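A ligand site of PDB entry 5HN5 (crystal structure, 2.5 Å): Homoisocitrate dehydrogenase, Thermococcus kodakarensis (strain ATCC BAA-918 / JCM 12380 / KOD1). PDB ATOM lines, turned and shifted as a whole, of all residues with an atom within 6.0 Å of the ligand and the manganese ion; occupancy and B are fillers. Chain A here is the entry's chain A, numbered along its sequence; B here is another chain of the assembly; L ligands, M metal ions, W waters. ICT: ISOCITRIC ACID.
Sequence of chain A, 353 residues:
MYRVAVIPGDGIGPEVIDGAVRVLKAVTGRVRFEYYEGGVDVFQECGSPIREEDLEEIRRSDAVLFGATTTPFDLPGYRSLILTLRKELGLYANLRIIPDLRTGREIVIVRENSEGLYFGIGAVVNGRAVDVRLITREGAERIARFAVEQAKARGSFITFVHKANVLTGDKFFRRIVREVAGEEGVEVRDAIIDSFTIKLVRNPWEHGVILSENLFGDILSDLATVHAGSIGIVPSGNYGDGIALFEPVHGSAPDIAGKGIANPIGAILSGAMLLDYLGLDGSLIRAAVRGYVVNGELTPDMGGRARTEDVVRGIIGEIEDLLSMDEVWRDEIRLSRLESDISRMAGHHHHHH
The side-chain carboxylate of Asp 218 is in salt-bridge range of the side-chain amino group of Lys 163 of chain B.
O of Asp 218 sits at hydrogen-bond distance from OG of Ser 221 (3.2 Å).
OD1 of Asp 194 of chain B is in salt-bridge range of NZ of Lys 163 of chain B (3.9 Å).
OH of Tyr 118 lies within hydrogen-bond range of NH1 of Arg 111 (3.1 Å).
The side-chain amide oxygen (OD1) of Asn 214 is in hydrogen-bond range of the guanidinium group (NE) of Arg 111, at 3.0 Å.
N of Arg 111 lies within hydrogen-bond range of O of Asn 94, at 2.7 Å.
The guanidinium group (NH2) of Arg 86 is in salt-bridge range of the side-chain carboxylate (OE1) of Glu 247.
The side-chain hydroxyl (OG) of Ser 80 lies within hydrogen-bond range of the backbone NH (N) of Leu 83.
Merely in contact with the ligand: Ile 82 and Leu 83.
Hydrophobic or aromatic side chains that line the ligand: Ile 82, Leu 83 and Tyr 118.
Within 4 Å of the ligand: Ser 80, Ile 82, Leu 83, Arg 86, Arg 96, Arg 111, Tyr 118, Asp 218, Lys 163 of chain B and Asp 194 of chain B.
The nearest printed residue that does not touch the ligand is Thr 71 (4.1 Å).
OD1 of Asp 218 is bound to the manganese ion.
Water W3 binds the manganese ion (2.1 Å).
OD2 of Asp 194 of chain B is bound to the manganese ion (2.1 Å).
The manganese ion is bound by O1 of the ligand (2.2 Å).
O7 of the ligand binds the manganese ion.
The manganese ion is bound by water W2, at 2.3 Å.
The manganese ion has six donor atoms within binding distance.
OH of Tyr 118 sits at hydrogen-bond distance from O5 of the ligand, 2.5 Å away.
O6 of the ligand is in salt-bridge range of NH1 of Arg 111 (2.6 Å).
An oxygen (O2) of the ligand lies within salt-bridge range of the guanidinium group of Arg 86 (2.8 Å).
O4 of the ligand sits at hydrogen-bond distance from OG of Ser 80 (3.1 Å).
NH2 of Arg 96 lies within salt-bridge range of O2 of the ligand (3.1 Å).
O5 of the ligand lies within salt-bridge range of NZ of Lys 163 of chain B.
Asp 222 touches the manganese ion (OD1 to MN, 3.9 Å).
NZ of Lys 163 of chain B touches the manganese ion (3.9 Å).
Four residues have an atom within 4 Å of the manganese ion: Asp 218, Asp 222, Lys 163 of chain B and Asp 194 of chain B.
The nearest printed residue that does not touch the manganese ion is Arg 96 (4.4 Å).
Water W3 lies within hydrogen-bond range of the side-chain carboxylate (OD1) of Asp 222 (2.5 Å), the backbone carbonyl oxygen (O) of Asp 218 (2.9 Å), the guanidinium group (NH1) of Arg 96 (3.1 Å) and the side-chain hydroxyl (OG) of Ser 221 (3.5 Å).
Water W1 lies within hydrogen-bond range of an oxygen (O4) of the ligand (2.4 Å), the side-chain hydroxyl of Thr 71 (2.7 Å) and the backbone carbonyl oxygen of Thr 69 (2.9 Å).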
ATOM      1  N   THR A  69     -16.846 -32.804  -7.957  1.00  0.00           N
ATOM      2  CA  THR A  69     -17.871 -33.789  -8.233  1.00  0.00           C
ATOM      3  C   THR A  69     -19.176 -33.080  -8.558  1.00  0.00           C
ATOM      4  O   THR A  69     -19.550 -32.084  -7.898  1.00  0.00           O
ATOM      5  CB  THR A  69     -18.045 -34.698  -6.998  1.00  0.00           C
ATOM      6  OG1 THR A  69     -18.937 -35.755  -7.300  1.00  0.00           O
ATOM      7  CG2 THR A  69     -18.581 -33.931  -5.761  1.00  0.00           C
ATOM      8  N   THR A  71     -22.948 -32.899  -8.278  1.00  0.00           N
ATOM      9  CA  THR A  71     -24.051 -33.494  -7.535  1.00  0.00           C
ATOM     10  C   THR A  71     -25.368 -33.057  -8.175  1.00  0.00           C
ATOM     11  O   THR A  71     -25.845 -31.957  -7.898  1.00  0.00           O
ATOM     12  CB  THR A  71     -23.987 -33.116  -6.031  1.00  0.00           C
ATOM     13  OG1 THR A  71     -22.892 -33.821  -5.421  1.00  0.00           O
ATOM     14  CG2 THR A  71     -25.324 -33.490  -5.311  1.00  0.00           C
ATOM     15  N   SER A  80     -24.055 -36.290  -2.389  1.00  0.00           N
ATOM     16  CA  SER A  80     -22.744 -35.708  -2.740  1.00  0.00           C
ATOM     17  C   SER A  80     -21.565 -36.582  -2.314  1.00  0.00           C
ATOM     18  O   SER A  80     -21.491 -37.044  -1.168  1.00  0.00           O
ATOM     19  CB  SER A  80     -22.600 -34.358  -2.036  1.00  0.00           C
ATOM     20  OG  SER A  80     -21.378 -33.701  -2.333  1.00  0.00           O
ATOM     21  N   ILE A  82     -18.403 -35.533  -1.905  1.00  0.00           N
ATOM     22  CA  ILE A  82     -17.596 -34.856  -0.884  1.00  0.00           C
ATOM     23  C   ILE A  82     -18.292 -34.897   0.468  1.00  0.00           C
ATOM     24  O   ILE A  82     -17.671 -35.215   1.504  1.00  0.00           O
ATOM     25  CB  ILE A  82     -17.099 -33.436  -1.304  1.00  0.00           C
ATOM     26  CG1 ILE A  82     -16.099 -32.892  -0.295  1.00  0.00           C
ATOM     27  CG2 ILE A  82     -18.221 -32.404  -1.466  1.00  0.00           C
ATOM     28  CD1 ILE A  82     -14.746 -33.563  -0.354  1.00  0.00           C
ATOM     29  N   LEU A  83     -19.602 -34.646   0.489  1.00  0.00           N
ATOM     30  CA  LEU A  83     -20.348 -34.716   1.773  1.00  0.00           C
ATOM     31  C   LEU A  83     -20.265 -36.132   2.388  1.00  0.00           C
ATOM     32  O   LEU A  83     -20.080 -36.299   3.592  1.00  0.00           O
ATOM     33  CB  LEU A  83     -21.798 -34.245   1.627  1.00  0.00           C
ATOM     34  CG  LEU A  83     -21.974 -32.772   1.192  1.00  0.00           C
ATOM     35  CD1 LEU A  83     -23.447 -32.453   0.994  1.00  0.00           C
ATOM     36  CD2 LEU A  83     -21.372 -31.818   2.210  1.00  0.00           C
ATOM     37  N   ARG A  86     -16.662 -36.641   3.720  1.00  0.00           N
ATOM     38  CA  ARG A  86     -16.551 -35.874   4.961  1.00  0.00           C
ATOM     39  C   ARG A  86     -17.057 -36.619   6.193  1.00  0.00           C
ATOM     40  O   ARG A  86     -16.453 -36.581   7.243  1.00  0.00           O
ATOM     41  CB  ARG A  86     -17.289 -34.537   4.843  1.00  0.00           C
ATOM     42  CG  ARG A  86     -16.542 -33.503   4.015  1.00  0.00           C
ATOM     43  CD  ARG A  86     -17.333 -32.210   3.845  1.00  0.00           C
ATOM     44  NE  ARG A  86     -16.717 -31.332   2.858  1.00  0.00           N
ATOM     45  CZ  ARG A  86     -17.336 -30.300   2.295  1.00  0.00           C
ATOM     46  NH1 ARG A  86     -18.599 -29.991   2.611  1.00  0.00           N
ATOM     47  NH2 ARG A  86     -16.699 -29.575   1.374  1.00  0.00           N
ATOM     48  N   ASN A  94     -13.150 -27.931   8.434  1.00  0.00           N
ATOM     49  CA  ASN A  94     -12.903 -27.470   7.076  1.00  0.00           C
ATOM     50  C   ASN A  94     -12.229 -26.121   7.172  1.00  0.00           C
ATOM     51  O   ASN A  94     -12.742 -25.216   7.847  1.00  0.00           O
ATOM     52  CB  ASN A  94     -14.221 -27.348   6.322  1.00  0.00           C
ATOM     53  CG  ASN A  94     -14.031 -27.056   4.839  1.00  0.00           C
ATOM     54  OD1 ASN A  94     -13.439 -26.048   4.462  1.00  0.00           O
ATOM     55  ND2 ASN A  94     -14.546 -27.943   3.992  1.00  0.00           N
ATOM     56  N   ARG A  96     -10.555 -23.026   4.945  1.00  0.00           N
ATOM     57  CA  ARG A  96     -10.500 -22.362   3.653  1.00  0.00           C
ATOM     58  C   ARG A  96      -9.732 -21.072   3.802  1.00  0.00           C
ATOM     59  O   ARG A  96      -9.954 -20.308   4.739  1.00  0.00           O
ATOM     60  CB  ARG A  96     -11.913 -22.107   3.139  1.00  0.00           C
ATOM     61  CG  ARG A  96     -12.546 -23.389   2.671  1.00  0.00           C
ATOM     62  CD  ARG A  96     -14.054 -23.332   2.533  1.00  0.00           C
ATOM     63  NE  ARG A  96     -14.506 -24.665   2.170  1.00  0.00           N
ATOM     64  CZ  ARG A  96     -15.585 -24.945   1.476  1.00  0.00           C
ATOM     65  NH1 ARG A  96     -16.417 -24.001   1.032  1.00  0.00           N
ATOM     66  NH2 ARG A  96     -15.844 -26.223   1.217  1.00  0.00           N
ATOM     67  N   ARG A 111     -14.639 -23.714   8.970  1.00  0.00           N
ATOM     68  CA  ARG A 111     -16.052 -24.106   8.902  1.00  0.00           C
ATOM     69  C   ARG A 111     -16.217 -25.424   9.639  1.00  0.00           C
ATOM     70  O   ARG A 111     -15.533 -26.388   9.300  1.00  0.00           O
ATOM     71  CB  ARG A 111     -16.487 -24.218   7.434  1.00  0.00           C
ATOM     72  CG  ARG A 111     -17.577 -25.213   7.141  1.00  0.00           C
ATOM     73  CD  ARG A 111     -17.794 -25.297   5.650  1.00  0.00           C
ATOM     74  NE  ARG A 111     -18.957 -26.109   5.357  1.00  0.00           N
ATOM     75  CZ  ARG A 111     -19.366 -26.416   4.135  1.00  0.00           C
ATOM     76  NH1 ARG A 111     -20.462 -27.131   3.960  1.00  0.00           N
ATOM     77  NH2 ARG A 111     -18.690 -26.001   3.070  1.00  0.00           N
ATOM     78  N   ASN A 113     -17.573 -28.958  10.129  1.00  0.00           N
ATOM     79  CA  ASN A 113     -17.752 -29.771   8.916  1.00  0.00           C
ATOM     80  C   ASN A 113     -18.498 -31.101   9.081  1.00  0.00           C
ATOM     81  O   ASN A 113     -18.628 -31.833   8.118  1.00  0.00           O
ATOM     82  CB  ASN A 113     -16.357 -30.067   8.379  1.00  0.00           C
ATOM     83  CG  ASN A 113     -16.308 -30.239   6.872  1.00  0.00           C
ATOM     84  OD1 ASN A 113     -16.965 -29.518   6.129  1.00  0.00           O
ATOM     85  ND2 ASN A 113     -15.468 -31.146   6.431  1.00  0.00           N
ATOM     86  N   TYR A 118     -25.962 -29.857   8.374  1.00  0.00           N
ATOM     87  CA  TYR A 118     -25.461 -31.050   7.649  1.00  0.00           C
ATOM     88  C   TYR A 118     -25.565 -32.361   8.455  1.00  0.00           C
ATOM     89  O   TYR A 118     -25.243 -33.422   7.929  1.00  0.00           O
ATOM     90  CB  TYR A 118     -23.984 -30.846   7.243  1.00  0.00           C
ATOM     91  CG  TYR A 118     -23.813 -29.869   6.113  1.00  0.00           C
ATOM     92  CD1 TYR A 118     -23.996 -28.502   6.317  1.00  0.00           C
ATOM     93  CD2 TYR A 118     -23.504 -30.294   4.828  1.00  0.00           C
ATOM     94  CE1 TYR A 118     -23.873 -27.589   5.269  1.00  0.00           C
ATOM     95  CE2 TYR A 118     -23.341 -29.384   3.794  1.00  0.00           C
ATOM     96  CZ  TYR A 118     -23.539 -28.052   4.013  1.00  0.00           C
ATOM     97  OH  TYR A 118     -23.391 -27.176   2.978  1.00  0.00           O
ATOM     98  N   ASN A 214     -21.494 -25.062  10.120  1.00  0.00           N
ATOM     99  CA  ASN A 214     -21.325 -25.710   8.805  1.00  0.00           C
ATOM    100  C   ASN A 214     -21.894 -24.896   7.654  1.00  0.00           C
ATOM    101  O   ASN A 214     -21.159 -24.413   6.793  1.00  0.00           O
ATOM    102  CB  ASN A 214     -21.952 -27.116   8.850  1.00  0.00           C
ATOM    103  CG  ASN A 214     -21.205 -28.159   7.987  1.00  0.00           C
ATOM    104  OD1 ASN A 214     -20.813 -27.919   6.836  1.00  0.00           O
ATOM    105  ND2 ASN A 214     -21.017 -29.325   8.553  1.00  0.00           N
ATOM    106  N   ASP A 218     -20.234 -22.512   4.908  1.00  0.00           N
ATOM    107  CA  ASP A 218     -20.354 -22.811   3.494  1.00  0.00           C
ATOM    108  C   ASP A 218     -20.639 -21.512   2.779  1.00  0.00           C
ATOM    109  O   ASP A 218     -20.022 -21.207   1.740  1.00  0.00           O
ATOM    110  CB  ASP A 218     -21.477 -23.834   3.285  1.00  0.00           C
ATOM    111  CG  ASP A 218     -21.786 -24.090   1.823  1.00  0.00           C
ATOM    112  OD1 ASP A 218     -20.903 -24.593   1.078  1.00  0.00           O
ATOM    113  OD2 ASP A 218     -22.953 -23.828   1.438  1.00  0.00           O
ATOM    114  N   ILE A 219     -21.566 -20.724   3.343  1.00  0.00           N
ATOM    115  CA  ILE A 219     -22.017 -19.496   2.740  1.00  0.00           C
ATOM    116  C   ILE A 219     -20.935 -18.408   2.786  1.00  0.00           C
ATOM    117  O   ILE A 219     -20.671 -17.775   1.787  1.00  0.00           O
ATOM    118  CB  ILE A 219     -23.270 -18.974   3.445  1.00  0.00           C
ATOM    119  CG1 ILE A 219     -24.449 -19.921   3.188  1.00  0.00           C
ATOM    120  CG2 ILE A 219     -23.608 -17.554   2.996  1.00  0.00           C
ATOM    121  CD1 ILE A 219     -25.689 -19.610   4.027  1.00  0.00           C
ATOM    122  N   SER A 221     -17.671 -18.723   3.071  1.00  0.00           N
ATOM    123  CA  SER A 221     -16.464 -19.077   2.315  1.00  0.00           C
ATOM    124  C   SER A 221     -16.591 -18.877   0.810  1.00  0.00           C
ATOM    125  O   SER A 221     -15.629 -18.522   0.148  1.00  0.00           O
ATOM    126  CB  SER A 221     -16.032 -20.521   2.632  1.00  0.00           C
ATOM    127  OG  SER A 221     -16.879 -21.464   2.006  1.00  0.00           O
ATOM    128  N   ASP A 222     -17.780 -19.090   0.271  1.00  0.00           N
ATOM    129  CA  ASP A 222     -18.058 -18.712  -1.124  1.00  0.00           C
ATOM    130  C   ASP A 222     -18.071 -17.180  -1.325  1.00  0.00           C
ATOM    131  O   ASP A 222     -17.609 -16.687  -2.359  1.00  0.00           O
ATOM    132  CB  ASP A 222     -19.389 -19.281  -1.580  1.00  0.00           C
ATOM    133  CG  ASP A 222     -19.245 -20.540  -2.369  1.00  0.00           C
ATOM    134  OD1 ASP A 222     -18.377 -21.376  -2.035  1.00  0.00           O
ATOM    135  OD2 ASP A 222     -20.013 -20.712  -3.331  1.00  0.00           O
ATOM    136  N   GLU A 247      -9.072 -30.332  -1.339  1.00  0.00           N
ATOM    137  CA  GLU A 247      -9.836 -30.113  -2.545  1.00  0.00           C
ATOM    138  C   GLU A 247      -9.896 -28.640  -2.775  1.00  0.00           C
ATOM    139  O   GLU A 247      -9.948 -27.875  -1.807  1.00  0.00           O
ATOM    140  CB  GLU A 247     -11.270 -30.598  -2.317  1.00  0.00           C
ATOM    141  CG  GLU A 247     -12.030 -29.795  -1.247  1.00  0.00           C
ATOM    142  CD  GLU A 247     -13.397 -30.324  -0.916  1.00  0.00           C
ATOM    143  OE1 GLU A 247     -13.802 -30.301   0.281  1.00  0.00           O
ATOM    144  OE2 GLU A 247     -14.077 -30.756  -1.874  1.00  0.00           O
ATOM    145  N   VAL A 249     -11.860 -25.253  -3.394  1.00  0.00           N
ATOM    146  CA  VAL A 249     -13.221 -24.847  -3.042  1.00  0.00           C
ATOM    147  C   VAL A 249     -14.150 -24.935  -4.240  1.00  0.00           C
ATOM    148  O   VAL A 249     -15.274 -25.360  -4.097  1.00  0.00           O
ATOM    149  CB  VAL A 249     -13.267 -23.454  -2.386  1.00  0.00           C
ATOM    150  CG1 VAL A 249     -14.709 -22.958  -2.241  1.00  0.00           C
ATOM    151  CG2 VAL A 249     -12.614 -23.531  -0.999  1.00  0.00           C
ATOM    152  N   LYS B 163     -30.703 -24.530  -0.499  1.00  0.00           N
ATOM    153  CA  LYS B 163     -29.723 -25.581  -0.325  1.00  0.00           C
ATOM    154  C   LYS B 163     -30.481 -26.928  -0.289  1.00  0.00           C
ATOM    155  O   LYS B 163     -30.279 -27.793   0.577  1.00  0.00           O
ATOM    156  CB  LYS B 163     -28.923 -25.373   0.965  1.00  0.00           C
ATOM    157  CG  LYS B 163     -27.604 -26.159   1.028  1.00  0.00           C
ATOM    158  CD  LYS B 163     -26.456 -25.501   0.238  1.00  0.00           C
ATOM    159  CE  LYS B 163     -25.190 -26.382   0.259  1.00  0.00           C
ATOM    160  NZ  LYS B 163     -23.924 -25.783  -0.286  1.00  0.00           N
ATOM    161  N   ASN B 165     -30.095 -29.464  -1.988  1.00  0.00           N
ATOM    162  CA  ASN B 165     -29.109 -30.559  -1.983  1.00  0.00           C
ATOM    163  C   ASN B 165     -28.824 -31.156  -0.604  1.00  0.00           C
ATOM    164  O   ASN B 165     -28.472 -32.318  -0.488  1.00  0.00           O
ATOM    165  CB  ASN B 165     -27.789 -30.121  -2.690  1.00  0.00           C
ATOM    166  CG  ASN B 165     -27.407 -28.637  -2.462  1.00  0.00           C
ATOM    167  OD1 ASN B 165     -28.261 -27.731  -2.381  1.00  0.00           O
ATOM    168  ND2 ASN B 165     -26.094 -28.372  -2.428  1.00  0.00           N
ATOM    169  N   VAL B 166     -28.936 -30.333   0.441  1.00  0.00           N
ATOM    170  CA  VAL B 166     -28.641 -30.725   1.815  1.00  0.00           C
ATOM    171  C   VAL B 166     -29.847 -30.674   2.725  1.00  0.00           C
ATOM    172  O   VAL B 166     -29.880 -31.421   3.715  1.00  0.00           O
ATOM    173  CB  VAL B 166     -27.602 -29.744   2.387  1.00  0.00           C
ATOM    174  CG1 VAL B 166     -27.476 -29.881   3.899  1.00  0.00           C
ATOM    175  CG2 VAL B 166     -26.260 -29.953   1.703  1.00  0.00           C
ATOM    176  N   ASP B 194     -24.916 -20.594  -1.398  1.00  0.00           N
ATOM    177  CA  ASP B 194     -23.481 -20.255  -1.282  1.00  0.00           C
ATOM    178  C   ASP B 194     -22.960 -19.581  -2.555  1.00  0.00           C
ATOM    179  O   ASP B 194     -22.392 -18.494  -2.486  1.00  0.00           O
ATOM    180  CB  ASP B 194     -22.616 -21.469  -0.879  1.00  0.00           C
ATOM    181  CG  ASP B 194     -22.846 -22.721  -1.766  1.00  0.00           C
ATOM    182  OD1 ASP B 194     -23.736 -22.724  -2.641  1.00  0.00           O
ATOM    183  OD2 ASP B 194     -22.139 -23.705  -1.554  1.00  0.00           O
ATOM    184  N   SER B 195     -23.161 -20.195  -3.718  1.00  0.00           N
ATOM    185  CA  SER B 195     -22.720 -19.573  -4.964  1.00  0.00           C
ATOM    186  C   SER B 195     -23.498 -18.289  -5.307  1.00  0.00           C
ATOM    187  O   SER B 195     -22.930 -17.345  -5.867  1.00  0.00           O
ATOM    188  CB  SER B 195     -22.803 -20.557  -6.122  1.00  0.00           C
ATOM    189  OG  SER B 195     -23.932 -21.385  -6.019  1.00  0.00           O
HETATM  190  C1  ICT L   1     -18.766 -27.024  -0.725  1.00  0.00           C
HETATM  191  O1  ICT L   1     -18.686 -25.837  -0.355  1.00  0.00           O
HETATM  192  O2  ICT L   1     -17.920 -27.871  -0.428  1.00  0.00           O
HETATM  193  C2  ICT L   1     -20.024 -27.515  -1.526  1.00  0.00           C
HETATM  194  O7  ICT L   1     -21.049 -26.468  -1.709  1.00  0.00           O
HETATM  195  C3  ICT L   1     -20.620 -28.685  -0.754  1.00  0.00           C
HETATM  196  C4  ICT L   1     -21.755 -29.459  -1.391  1.00  0.00           C
HETATM  197  C5  ICT L   1     -21.596 -29.632  -2.890  1.00  0.00           C
HETATM  198  O3  ICT L   1     -21.962 -28.669  -3.610  1.00  0.00           O
HETATM  199  O4  ICT L   1     -21.154 -30.756  -3.270  1.00  0.00           O
HETATM  200  C6  ICT L   1     -21.098 -28.232   0.659  1.00  0.00           C
HETATM  201  O5  ICT L   1     -22.342 -28.206   0.904  1.00  0.00           O
HETATM  202  O6  ICT L   1     -20.205 -28.001   1.493  1.00  0.00           O
HETATM  203 MN    MN M   1     -20.332 -24.501  -0.903  1.00  0.00          MN
HETATM  204  O   HOH W   1     -21.168 -31.716  -5.482  1.00  0.00           O
HETATM  205  O   HOH W   2     -19.149 -23.965  -2.800  1.00  0.00           O
HETATM  206  O   HOH W   3     -19.008 -23.031  -0.272  1.00  0.00           O
